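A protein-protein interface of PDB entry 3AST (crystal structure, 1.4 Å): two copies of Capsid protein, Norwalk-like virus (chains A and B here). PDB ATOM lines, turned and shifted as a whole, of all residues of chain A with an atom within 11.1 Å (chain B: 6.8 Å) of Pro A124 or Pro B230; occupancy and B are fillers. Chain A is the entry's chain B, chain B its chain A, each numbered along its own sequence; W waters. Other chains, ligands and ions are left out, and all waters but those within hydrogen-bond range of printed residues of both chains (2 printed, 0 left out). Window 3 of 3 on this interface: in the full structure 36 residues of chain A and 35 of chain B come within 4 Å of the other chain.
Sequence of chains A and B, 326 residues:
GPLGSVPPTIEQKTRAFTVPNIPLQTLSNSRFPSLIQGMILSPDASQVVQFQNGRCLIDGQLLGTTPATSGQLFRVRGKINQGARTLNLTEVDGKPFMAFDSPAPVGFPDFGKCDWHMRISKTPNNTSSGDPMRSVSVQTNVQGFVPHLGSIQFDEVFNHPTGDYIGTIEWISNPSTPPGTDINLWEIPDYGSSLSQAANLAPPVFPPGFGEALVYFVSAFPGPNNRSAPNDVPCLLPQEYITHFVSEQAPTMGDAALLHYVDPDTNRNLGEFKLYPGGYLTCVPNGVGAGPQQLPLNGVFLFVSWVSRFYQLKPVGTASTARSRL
O of Ala B229 is in hydrogen-bond range of ND2 of Asn A125 (2.8 Å).
The backbone NH (N) of Asn B225 is in hydrogen-bond range of the backbone carbonyl oxygen (O) of Thr A127 (3.3 Å).
The side-chain amide oxygen (OD1) of Asn B225 sits at hydrogen-bond distance from the backbone NH (N) of Arg B227.
ND2 of Asn A125 is in hydrogen-bond range of O of Thr A127, 2.9 Å away.
OG1 of Thr A127 sits at hydrogen-bond distance from N of Ser A129, at 3.3 Å.
OD1 of Asn B225 is in hydrogen-bond range of N of Ser B228.
The side-chain amino group (NZ) of Lys A122 lies close to the side-chain amide nitrogen (ND2) of Asn A126 (3.3 Å).
The side-chain amide nitrogen (ND2) of Asn B231 lies close to the side-chain amide nitrogen (ND2) of Asn B225 (2.9 Å).
Among the printed residues, merely in contact across the chains: Pro A124 with Pro B230, Asn A125 with Gly B223, Asn A125 with Asn B225, Asn A125 with Ser B228, Asn A125 with Pro B230, Asn A126 with Ser B228, Thr A127 with Ser B228, Ser A128 with Asn B225 and Ser A128 with Ser B228.
Of chain B, only Pro B230 comes within 4 Å of Pro A124.
Of the printed residues of chain B, Asn A125 touches Gly B223 (3.3 Å), Asn B225 (3.7 Å), Ser B228 (3.6 Å), Ala B229 (2.8 Å) and Pro B230 (3.7 Å).
Printed residues of chain B within 4 Å of Asn A126: Ser B228.
Printed residues of chain B within 4 Å of Ser A128: Asn B225 and Ser B228.
Of the printed residues of chain A, Asn B225 touches Asn A125, Thr A127 and Ser A128.
Of chain A, only Asn A125 comes within 4 Å of Ala B229.
Of the printed residues of chain A, Pro B230 touches Pro A124 and Asn A125.
No residue of chain A comes within 4 Å of Asp B232.
The nearest printed residue of chain B that does not touch Pro A124 is Ala B229 (6.0 Å).
The nearest residue of chain A that does not touch Pro B230 is Asn A126 (5.7 Å).
The nearest printed residue of chain B that does not touch Asn A125 is Asn B231 (5.1 Å).
Printed residues of chain A that touch a printed residue of chain B: Pro A124, Asn A125, Asn A126, Thr A127 and Ser A128.
Along chain A the printed residues that touch a printed residue of chain B span positions 124 to 128.
Hydrophobic or aromatic side chains of chain B that line the printed part of chain A: Pro B230.
Among the printed residues, 11 pairs touch across the chains.
Among the printed residues, no Asp or Glu carboxylate lies within 4 Å of a Lys or Arg side-chain nitrogen of the other chain.
No position is printed for both chains.
Water W2 lies within hydrogen-bond range of OG1 of Thr A123 (3.0 Å) and NE2 of Gln B37 (3.2 Å).
Water W1 lies within hydrogen-bond range of the side-chain amide nitrogen of Gln B37 and the backbone carbonyl oxygen of Asp A93.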
ATOM      1  N   ARG A  77       7.988   8.536  32.721  1.00  0.00           N
ATOM      2  CA  ARG A  77       9.239   9.249  32.491  1.00  0.00           C
ATOM      3  C   ARG A  77      10.022   9.358  33.784  1.00  0.00           C
ATOM      4  O   ARG A  77       9.453   9.571  34.851  1.00  0.00           O
ATOM      5  CB  ARG A  77       8.977  10.640  31.912  1.00  0.00           C
ATOM      6  CG  ARG A  77      10.252  11.399  31.538  1.00  0.00           C
ATOM      7  CD  ARG A  77       9.948  12.649  30.748  1.00  0.00           C
ATOM      8  NE  ARG A  77      11.164  13.359  30.353  1.00  0.00           N
ATOM      9  CZ  ARG A  77      11.190  14.381  29.502  1.00  0.00           C
ATOM     10  NH1 ARG A  77      10.065  14.821  28.947  1.00  0.00           N
ATOM     11  NH2 ARG A  77      12.346  14.966  29.205  1.00  0.00           N
ATOM     12  N   GLY A  78      11.336   9.211  33.675  1.00  0.00           N
ATOM     13  CA  GLY A  78      12.206   9.415  34.821  1.00  0.00           C
ATOM     14  C   GLY A  78      13.673   9.332  34.471  1.00  0.00           C
ATOM     15  O   GLY A  78      14.042   9.125  33.311  1.00  0.00           O
ATOM     16  N   LYS A  79      14.505   9.508  35.492  1.00  0.00           N
ATOM     17  CA  LYS A  79      15.950   9.393  35.354  1.00  0.00           C
ATOM     18  C   LYS A  79      16.401   8.040  35.872  1.00  0.00           C
ATOM     19  O   LYS A  79      15.922   7.573  36.904  1.00  0.00           O
ATOM     20  CB  LYS A  79      16.664  10.492  36.152  1.00  0.00           C
ATOM     21  CG  LYS A  79      16.190  11.919  35.900  1.00  0.00           C
ATOM     22  CD  LYS A  79      16.423  12.360  34.463  1.00  0.00           C
ATOM     23  CE  LYS A  79      16.301  13.875  34.318  1.00  0.00           C
ATOM     24  NZ  LYS A  79      14.928  14.369  34.620  1.00  0.00           N
ATOM     25  N   THR A  90       9.726  11.569  36.921  1.00  0.00           N
ATOM     26  CA  THR A  90       9.351  12.963  36.745  1.00  0.00           C
ATOM     27  C   THR A  90       7.961  12.986  36.128  1.00  0.00           C
ATOM     28  O   THR A  90       7.394  11.930  35.825  1.00  0.00           O
ATOM     29  CB  THR A  90      10.332  13.714  35.808  1.00  0.00           C
ATOM     30  OG1 THR A  90      10.306  13.122  34.503  1.00  0.00           O
ATOM     31  CG2 THR A  90      11.754  13.691  36.363  1.00  0.00           C
ATOM     32  N   VAL A  92       5.579  13.712  32.842  1.00  0.00           N
ATOM     33  CA  VAL A  92       5.787  13.321  31.446  1.00  0.00           C
ATOM     34  C   VAL A  92       6.535  14.385  30.626  1.00  0.00           C
ATOM     35  O   VAL A  92       7.304  14.048  29.725  1.00  0.00           O
ATOM     36  CB  VAL A  92       4.443  12.916  30.776  1.00  0.00           C
ATOM     37  CG1 VAL A  92       4.616  12.638  29.285  1.00  0.00           C
ATOM     38  CG2 VAL A  92       3.856  11.690  31.470  1.00  0.00           C
ATOM     39  N   ASP A  93       6.331  15.660  30.953  1.00  0.00           N
ATOM     40  CA  ASP A  93       7.034  16.737  30.249  1.00  0.00           C
ATOM     41  C   ASP A  93       8.427  17.034  30.823  1.00  0.00           C
ATOM     42  O   ASP A  93       9.111  17.951  30.364  1.00  0.00           O
ATOM     43  CB  ASP A  93       6.171  18.007  30.158  1.00  0.00           C
ATOM     44  CG  ASP A  93       5.972  18.700  31.499  1.00  0.00           C
ATOM     45  OD1 ASP A  93       6.272  18.112  32.562  1.00  0.00           O
ATOM     46  OD2 ASP A  93       5.495  19.855  31.487  1.00  0.00           O
ATOM     47  N   GLY A  94       8.842  16.256  31.822  1.00  0.00           N
ATOM     48  CA  GLY A  94      10.187  16.367  32.390  1.00  0.00           C
ATOM     49  C   GLY A  94      10.272  17.178  33.669  1.00  0.00           C
ATOM     50  O   GLY A  94      11.305  17.171  34.340  1.00  0.00           O
ATOM     51  N   ILE A 120      11.185   1.815  26.509  1.00  0.00           N
ATOM     52  CA  ILE A 120      11.611   3.167  26.867  1.00  0.00           C
ATOM     53  C   ILE A 120      12.811   3.582  26.017  1.00  0.00           C
ATOM     54  O   ILE A 120      13.510   2.732  25.460  1.00  0.00           O
ATOM     55  CB  ILE A 120      11.945   3.298  28.386  1.00  0.00           C
ATOM     56  CG1 ILE A 120      13.130   2.398  28.784  1.00  0.00           C
ATOM     57  CG2 ILE A 120      10.700   3.019  29.241  1.00  0.00           C
ATOM     58  CD1 ILE A 120      13.619   2.594  30.223  1.00  0.00           C
ATOM     59  N   SER A 121      13.039   4.887  25.908  1.00  0.00           N
ATOM     60  CA  SER A 121      14.193   5.405  25.179  1.00  0.00           C
ATOM     61  C   SER A 121      14.681   6.700  25.810  1.00  0.00           C
ATOM     62  O   SER A 121      13.907   7.426  26.435  1.00  0.00           O
ATOM     63  CB  SER A 121      13.867   5.600  23.692  1.00  0.00           C
ATOM     64  OG  SER A 121      12.937   6.650  23.495  1.00  0.00           O
ATOM     65  N   LYS A 122      15.975   6.969  25.648  1.00  0.00           N
ATOM     66  CA  LYS A 122      16.610   8.162  26.195  1.00  0.00           C
ATOM     67  C   LYS A 122      16.183   9.385  25.393  1.00  0.00           C
ATOM     68  O   LYS A 122      16.188   9.360  24.158  1.00  0.00           O
ATOM     69  CB  LYS A 122      18.134   7.999  26.174  1.00  0.00           C
ATOM     70  CG  LYS A 122      18.914   9.074  26.921  1.00  0.00           C
ATOM     71  CD  LYS A 122      20.396   8.704  27.018  1.00  0.00           C
ATOM     72  CE  LYS A 122      21.243   9.878  27.485  1.00  0.00           C
ATOM     73  NZ  LYS A 122      21.387  10.915  26.429  1.00  0.00           N
ATOM     74  N   THR A 123      15.809  10.447  26.101  1.00  0.00           N
ATOM     75  CA  THR A 123      15.290  11.656  25.473  1.00  0.00           C
ATOM     76  C   THR A 123      15.960  12.911  26.060  1.00  0.00           C
ATOM     77  O   THR A 123      16.286  12.933  27.247  1.00  0.00           O
ATOM     78  CB  THR A 123      13.735  11.715  25.581  1.00  0.00           C
ATOM     79  OG1 THR A 123      13.214  12.680  24.660  1.00  0.00           O
ATOM     80  CG2 THR A 123      13.272  12.044  27.006  1.00  0.00           C
ATOM     81  N   PRO A 124      16.216  13.938  25.223  1.00  0.00           N
ATOM     82  CA  PRO A 124      16.033  13.968  23.775  1.00  0.00           C
ATOM     83  C   PRO A 124      17.124  13.177  23.073  1.00  0.00           C
ATOM     84  O   PRO A 124      18.172  12.912  23.671  1.00  0.00           O
ATOM     85  CB  PRO A 124      16.177  15.455  23.443  1.00  0.00           C
ATOM     86  CG  PRO A 124      17.105  15.971  24.471  1.00  0.00           C
ATOM     87  CD  PRO A 124      16.761  15.216  25.726  1.00  0.00           C
ATOM     88  N   ASN A 125      16.885  12.799  21.823  1.00  0.00           N
ATOM     89  CA  ASN A 125      17.944  12.192  21.033  1.00  0.00           C
ATOM     90  C   ASN A 125      19.141  13.129  20.960  1.00  0.00           C
ATOM     91  O   ASN A 125      18.988  14.333  20.728  1.00  0.00           O
ATOM     92  CB  ASN A 125      17.496  11.866  19.611  1.00  0.00           C
ATOM     93  CG  ASN A 125      18.651  11.388  18.755  1.00  0.00           C
ATOM     94  OD1 ASN A 125      19.236  10.339  19.024  1.00  0.00           O
ATOM     95  ND2 ASN A 125      19.026  12.178  17.762  1.00  0.00           N
ATOM     96  N   ASN A 126      20.328  12.560  21.150  1.00  0.00           N
ATOM     97  CA  ASN A 126      21.572  13.310  21.026  1.00  0.00           C
ATOM     98  C   ASN A 126      22.617  12.556  20.192  1.00  0.00           C
ATOM     99  O   ASN A 126      23.813  12.813  20.308  1.00  0.00           O
ATOM    100  CB  ASN A 126      22.114  13.683  22.414  1.00  0.00           C
ATOM    101  CG  ASN A 126      22.591  12.476  23.213  1.00  0.00           C
ATOM    102  OD1 ASN A 126      22.423  11.329  22.802  1.00  0.00           O
ATOM    103  ND2 ASN A 126      23.201  12.741  24.363  1.00  0.00           N
ATOM    104  N   THR A 127      22.153  11.644  19.340  1.00  0.00           N
ATOM    105  CA  THR A 127      23.044  10.774  18.561  1.00  0.00           C
ATOM    106  C   THR A 127      22.615  10.605  17.101  1.00  0.00           C
ATOM    107  O   THR A 127      21.461  10.875  16.739  1.00  0.00           O
ATOM    108  CB  THR A 127      23.225   9.381  19.243  1.00  0.00           C
ATOM    109  OG1 THR A 127      24.181   8.597  18.515  1.00  0.00           O
ATOM    110  CG2 THR A 127      21.913   8.607  19.320  1.00  0.00           C
ATOM    111  N   SER A 128      23.557  10.160  16.272  1.00  0.00           N
ATOM    112  CA  SER A 128      23.323   9.943  14.844  1.00  0.00           C
ATOM    113  C   SER A 128      23.188   8.467  14.471  1.00  0.00           C
ATOM    114  O   SER A 128      22.951   8.140  13.309  1.00  0.00           O
ATOM    115  CB  SER A 128      24.447  10.581  14.019  1.00  0.00           C
ATOM    116  OG  SER A 128      25.681   9.934  14.272  1.00  0.00           O
ATOM    117  N   SER A 129      23.331   7.581  15.454  1.00  0.00           N
ATOM    118  CA  SER A 129      23.365   6.149  15.176  1.00  0.00           C
ATOM    119  C   SER A 129      22.613   5.311  16.199  1.00  0.00           C
ATOM    120  O   SER A 129      22.544   5.660  17.378  1.00  0.00           O
ATOM    121  CB  SER A 129      24.818   5.670  15.105  1.00  0.00           C
ATOM    122  OG  SER A 129      25.448   5.810  16.359  1.00  0.00           O
ATOM    123  N   PRO A 132      17.384   3.123  19.630  1.00  0.00           N
ATOM    124  CA  PRO A 132      17.327   3.714  20.969  1.00  0.00           C
ATOM    125  C   PRO A 132      16.431   2.959  21.960  1.00  0.00           C
ATOM    126  O   PRO A 132      16.402   3.301  23.143  1.00  0.00           O
ATOM    127  CB  PRO A 132      16.738   5.097  20.696  1.00  0.00           C
ATOM    128  CG  PRO A 132      15.800   4.857  19.556  1.00  0.00           C
ATOM    129  CD  PRO A 132      16.457   3.795  18.698  1.00  0.00           C
ATOM    130  N   ARG A 134      14.688   0.346  24.506  1.00  0.00           N
ATOM    131  CA  ARG A 134      15.078  -0.586  25.562  1.00  0.00           C
ATOM    132  C   ARG A 134      13.850  -1.263  26.158  1.00  0.00           C
ATOM    133  O   ARG A 134      12.830  -0.613  26.403  1.00  0.00           O
ATOM    134  CB  ARG A 134      15.852   0.137  26.672  1.00  0.00           C
ATOM    135  CG  ARG A 134      16.968   1.075  26.193  1.00  0.00           C
ATOM    136  CD  ARG A 134      18.163   0.324  25.609  1.00  0.00           C
ATOM    137  NE  ARG A 134      19.118   1.242  24.983  1.00  0.00           N
ATOM    138  CZ  ARG A 134      19.354   1.326  23.672  1.00  0.00           C
ATOM    139  NH1 ARG A 134      18.716   0.539  22.811  1.00  0.00           N
ATOM    140  NH2 ARG A 134      20.240   2.204  23.219  1.00  0.00           N
ATOM    141  N   PRO A 161      22.921   3.256  28.884  1.00  0.00           N
ATOM    142  CA  PRO A 161      23.387   4.596  29.235  1.00  0.00           C
ATOM    143  C   PRO A 161      22.501   5.366  30.218  1.00  0.00           C
ATOM    144  O   PRO A 161      21.268   5.301  30.146  1.00  0.00           O
ATOM    145  CB  PRO A 161      23.440   5.308  27.881  1.00  0.00           C
ATOM    146  CG  PRO A 161      23.757   4.218  26.929  1.00  0.00           C
ATOM    147  CD  PRO A 161      23.003   3.022  27.429  1.00  0.00           C
ATOM    148  N   THR A 162      23.153   6.070  31.137  1.00  0.00           N
ATOM    149  CA  THR A 162      22.500   6.959  32.087  1.00  0.00           C
ATOM    150  C   THR A 162      21.730   8.052  31.356  1.00  0.00           C
ATOM    151  O   THR A 162      22.207   8.594  30.357  1.00  0.00           O
ATOM    152  CB  THR A 162      23.554   7.610  33.011  1.00  0.00           C
ATOM    153  OG1 THR A 162      24.181   6.591  33.797  1.00  0.00           O
ATOM    154  CG2 THR A 162      22.934   8.657  33.930  1.00  0.00           C
ATOM    155  N   GLY A 163      20.532   8.363  31.845  1.00  0.00           N
ATOM    156  CA  GLY A 163      19.791   9.490  31.308  1.00  0.00           C
ATOM    157  C   GLY A 163      18.323   9.580  31.660  1.00  0.00           C
ATOM    158  O   GLY A 163      17.829   8.905  32.567  1.00  0.00           O
ATOM    159  N   ASP A 164      17.654  10.454  30.918  1.00  0.00           N
ATOM    160  CA  ASP A 164      16.237  10.749  31.026  1.00  0.00           C
ATOM    161  C   ASP A 164      15.518   9.833  30.042  1.00  0.00           C
ATOM    162  O   ASP A 164      15.743   9.922  28.832  1.00  0.00           O
ATOM    163  CB  ASP A 164      16.056  12.219  30.637  1.00  0.00           C
ATOM    164  CG  ASP A 164      14.647  12.744  30.840  1.00  0.00           C
ATOM    165  OD1 ASP A 164      13.702  11.967  31.087  1.00  0.00           O
ATOM    166  OD2 ASP A 164      14.493  13.980  30.730  1.00  0.00           O
ATOM    167  N   TYR A 165      14.672   8.946  30.560  1.00  0.00           N
ATOM    168  CA  TYR A 165      13.973   7.969  29.726  1.00  0.00           C
ATOM    169  C   TYR A 165      12.471   8.177  29.735  1.00  0.00           C
ATOM    170  O   TYR A 165      11.884   8.495  30.767  1.00  0.00           O
ATOM    171  CB  TYR A 165      14.294   6.538  30.168  1.00  0.00           C
ATOM    172  CG  TYR A 165      15.653   6.056  29.719  1.00  0.00           C
ATOM    173  CD1 TYR A 165      15.786   5.239  28.600  1.00  0.00           C
ATOM    174  CD2 TYR A 165      16.806   6.421  30.413  1.00  0.00           C
ATOM    175  CE1 TYR A 165      17.034   4.790  28.178  1.00  0.00           C
ATOM    176  CE2 TYR A 165      18.056   5.982  29.999  1.00  0.00           C
ATOM    177  CZ  TYR A 165      18.162   5.168  28.883  1.00  0.00           C
ATOM    178  OH  TYR A 165      19.397   4.729  28.468  1.00  0.00           O
ATOM    179  N   ILE A 166      11.867   7.994  28.565  1.00  0.00           N
ATOM    180  CA  ILE A 166      10.419   8.069  28.404  1.00  0.00           C
ATOM    181  C   ILE A 166       9.933   6.815  27.689  1.00  0.00           C
ATOM    182  O   ILE A 166      10.605   6.284  26.805  1.00  0.00           O
ATOM    183  CB  ILE A 166       9.981   9.342  27.614  1.00  0.00           C
ATOM    184  CG1 ILE A 166       8.459   9.394  27.431  1.00  0.00           C
ATOM    185  CG2 ILE A 166      10.643   9.402  26.242  1.00  0.00           C
ATOM    186  CD1 ILE A 166       7.698   9.923  28.597  1.00  0.00           C
ATOM    187  N   GLY A 167       8.756   6.346  28.074  1.00  0.00           N
ATOM    188  CA  GLY A 167       8.142   5.236  27.381  1.00  0.00           C
ATOM    189  C   GLY A 167       6.791   4.889  27.945  1.00  0.00           C
ATOM    190  O   GLY A 167       6.128   5.717  28.580  1.00  0.00           O
ATOM    191  N   GLN B  37       5.385  20.098  22.196  1.00  0.00           N
ATOM    192  CA  GLN B  37       6.564  20.572  22.916  1.00  0.00           C
ATOM    193  C   GLN B  37       7.032  21.953  22.468  1.00  0.00           C
ATOM    194  O   GLN B  37       7.901  22.551  23.102  1.00  0.00           O
ATOM    195  CB  GLN B  37       7.706  19.572  22.774  1.00  0.00           C
ATOM    196  CG  GLN B  37       7.465  18.269  23.501  1.00  0.00           C
ATOM    197  CD  GLN B  37       8.588  17.293  23.281  1.00  0.00           C
ATOM    198  OE1 GLN B  37       8.783  16.802  22.173  1.00  0.00           O
ATOM    199  NE2 GLN B  37       9.347  17.012  24.336  1.00  0.00           N
ATOM    200  N   LEU B 185      10.894  15.104   7.980  1.00  0.00           N
ATOM    201  CA  LEU B 185       9.522  14.965   8.460  1.00  0.00           C
ATOM    202  C   LEU B 185       8.580  16.045   7.929  1.00  0.00           C
ATOM    203  O   LEU B 185       7.387  16.036   8.235  1.00  0.00           O
ATOM    204  CB  LEU B 185       9.494  14.908   9.991  1.00  0.00           C
ATOM    205  CG  LEU B 185      10.094  13.625  10.580  1.00  0.00           C
ATOM    206  CD1 LEU B 185      10.514  13.849  12.027  1.00  0.00           C
ATOM    207  CD2 LEU B 185       9.127  12.450  10.455  1.00  0.00           C
ATOM    208  N   SER B 219       6.557  17.868  18.171  1.00  0.00           N
ATOM    209  CA  SER B 219       6.816  16.906  19.236  1.00  0.00           C
ATOM    210  C   SER B 219       7.952  16.001  18.790  1.00  0.00           C
ATOM    211  O   SER B 219       8.021  15.626  17.617  1.00  0.00           O
ATOM    212  CB  SER B 219       5.575  16.062  19.518  1.00  0.00           C
ATOM    213  OG  SER B 219       4.437  16.877  19.743  1.00  0.00           O
ATOM    214  N   ALA B 220       8.833  15.643  19.722  1.00  0.00           N
ATOM    215  CA  ALA B 220       9.959  14.764  19.420  1.00  0.00           C
ATOM    216  C   ALA B 220       9.508  13.317  19.261  1.00  0.00           C
ATOM    217  O   ALA B 220       8.751  12.802  20.080  1.00  0.00           O
ATOM    218  CB  ALA B 220      11.014  14.869  20.508  1.00  0.00           C
ATOM    219  N   PHE B 221       9.978  12.676  18.194  1.00  0.00           N
ATOM    220  CA  PHE B 221       9.704  11.270  17.936  1.00  0.00           C
ATOM    221  C   PHE B 221      11.007  10.477  18.045  1.00  0.00           C
ATOM    222  O   PHE B 221      12.030  10.927  17.532  1.00  0.00           O
ATOM    223  CB  PHE B 221       9.100  11.091  16.541  1.00  0.00           C
ATOM    224  CG  PHE B 221       8.505   9.739  16.325  1.00  0.00           C
ATOM    225  CD1 PHE B 221       7.190   9.489  16.690  1.00  0.00           C
ATOM    226  CD2 PHE B 221       9.266   8.702  15.795  1.00  0.00           C
ATOM    227  CE1 PHE B 221       6.635   8.233  16.527  1.00  0.00           C
ATOM    228  CE2 PHE B 221       8.717   7.435  15.626  1.00  0.00           C
ATOM    229  CZ  PHE B 221       7.399   7.199  15.990  1.00  0.00           C
ATOM    230  N   GLY B 223      14.321   8.312  17.777  1.00  0.00           N
ATOM    231  CA  GLY B 223      15.219   7.919  16.713  1.00  0.00           C
ATOM    232  C   GLY B 223      16.386   8.870  16.546  1.00  0.00           C
ATOM    233  O   GLY B 223      16.315  10.033  16.946  1.00  0.00           O
ATOM    234  N   ASN B 225      19.350  11.003  14.226  1.00  0.00           N
ATOM    235  CA  ASN B 225      19.439  11.709  12.950  1.00  0.00           C
ATOM    236  C   ASN B 225      20.821  12.330  12.785  1.00  0.00           C
ATOM    237  O   ASN B 225      21.610  12.351  13.732  1.00  0.00           O
ATOM    238  CB  ASN B 225      18.314  12.750  12.778  1.00  0.00           C
ATOM    239  CG  ASN B 225      18.358  13.855  13.818  1.00  0.00           C
ATOM    240  OD1 ASN B 225      19.421  14.365  14.171  1.00  0.00           O
ATOM    241  ND2 ASN B 225      17.185  14.256  14.294  1.00  0.00           N
ATOM    242  N   ARG B 227      21.931  15.236  12.677  1.00  0.00           N
ATOM    243  CA  ARG B 227      22.222  16.425  13.475  1.00  0.00           C
ATOM    244  C   ARG B 227      22.385  16.119  14.968  1.00  0.00           C
ATOM    245  O   ARG B 227      22.629  17.028  15.765  1.00  0.00           O
ATOM    246  CB  ARG B 227      21.128  17.483  13.275  1.00  0.00           C
ATOM    247  CG  ARG B 227      20.901  17.886  11.821  1.00  0.00           C
ATOM    248  CD  ARG B 227      19.787  18.926  11.665  1.00  0.00           C
ATOM    249  NE  ARG B 227      18.586  18.612  12.441  1.00  0.00           N
ATOM    250  CZ  ARG B 227      17.643  17.743  12.076  1.00  0.00           C
ATOM    251  NH1 ARG B 227      17.743  17.072  10.935  1.00  0.00           N
ATOM    252  NH2 ARG B 227      16.597  17.541  12.863  1.00  0.00           N
ATOM    253  N   SER B 228      22.249  14.841  15.338  1.00  0.00           N
ATOM    254  CA  SER B 228      22.269  14.405  16.743  1.00  0.00           C
ATOM    255  C   SER B 228      21.299  15.239  17.585  1.00  0.00           C
ATOM    256  O   SER B 228      21.619  15.678  18.690  1.00  0.00           O
ATOM    257  CB  SER B 228      23.692  14.441  17.316  1.00  0.00           C
ATOM    258  OG  SER B 228      24.525  13.524  16.626  1.00  0.00           O
ATOM    259  N   ALA B 229      20.106  15.444  17.034  1.00  0.00           N
ATOM    260  CA  ALA B 229      19.084  16.278  17.650  1.00  0.00           C
ATOM    261  C   ALA B 229      17.754  15.524  17.626  1.00  0.00           C
ATOM    262  O   ALA B 229      17.646  14.509  16.946  1.00  0.00           O
ATOM    263  CB  ALA B 229      18.974  17.598  16.898  1.00  0.00           C
ATOM    264  N   PRO B 230      16.743  16.002  18.380  1.00  0.00           N
ATOM    265  CA  PRO B 230      15.445  15.319  18.316  1.00  0.00           C
ATOM    266  C   PRO B 230      14.827  15.342  16.915  1.00  0.00           C
ATOM    267  O   PRO B 230      14.959  16.334  16.191  1.00  0.00           O
ATOM    268  CB  PRO B 230      14.568  16.122  19.283  1.00  0.00           C
ATOM    269  CG  PRO B 230      15.509  16.854  20.161  1.00  0.00           C
ATOM    270  CD  PRO B 230      16.761  17.080  19.386  1.00  0.00           C
ATOM    271  N   ASN B 231      14.176  14.243  16.543  1.00  0.00           N
ATOM    272  CA  ASN B 231      13.325  14.211  15.356  1.00  0.00           C
ATOM    273  C   ASN B 231      12.003  14.907  15.663  1.00  0.00           C
ATOM    274  O   ASN B 231      11.063  14.283  16.161  1.00  0.00           O
ATOM    275  CB  ASN B 231      13.056  12.767  14.915  1.00  0.00           C
ATOM    276  CG  ASN B 231      14.252  12.113  14.250  1.00  0.00           C
ATOM    277  OD1 ASN B 231      14.622  10.984  14.585  1.00  0.00           O
ATOM    278  ND2 ASN B 231      14.852  12.805  13.298  1.00  0.00           N
ATOM    279  N   ASP B 232      11.938  16.204  15.378  1.00  0.00           N
ATOM    280  CA  ASP B 232      10.741  16.984  15.668  1.00  0.00           C
ATOM    281  C   ASP B 232       9.712  16.829  14.550  1.00  0.00           C
ATOM    282  O   ASP B 232      10.007  17.073  13.377  1.00  0.00           O
ATOM    283  CB  ASP B 232      11.092  18.451  15.922  1.00  0.00           C
ATOM    284  CG  ASP B 232      11.757  18.671  17.278  1.00  0.00           C
ATOM    285  OD1 ASP B 232      11.515  17.886  18.225  1.00  0.00           O
ATOM    286  OD2 ASP B 232      12.525  19.648  17.403  1.00  0.00           O
ATOM    287  N   VAL B 233       8.516  16.389  14.927  1.00  0.00           N
ATOM    288  CA  VAL B 233       7.443  16.148  13.971  1.00  0.00           C
ATOM    289  C   VAL B 233       6.524  17.364  13.954  1.00  0.00           C
ATOM    290  O   VAL B 233       5.868  17.647  14.961  1.00  0.00           O
ATOM    291  CB  VAL B 233       6.620  14.894  14.343  1.00  0.00           C
ATOM    292  CG1 VAL B 233       5.473  14.687  13.360  1.00  0.00           C
ATOM    293  CG2 VAL B 233       7.502  13.656  14.385  1.00  0.00           C
HETATM  294  O   HOH W   1       8.723  17.878  27.169  1.00  0.00           O
HETATM  295  O   HOH W   2      12.176  15.501  24.379  1.00  0.00           O
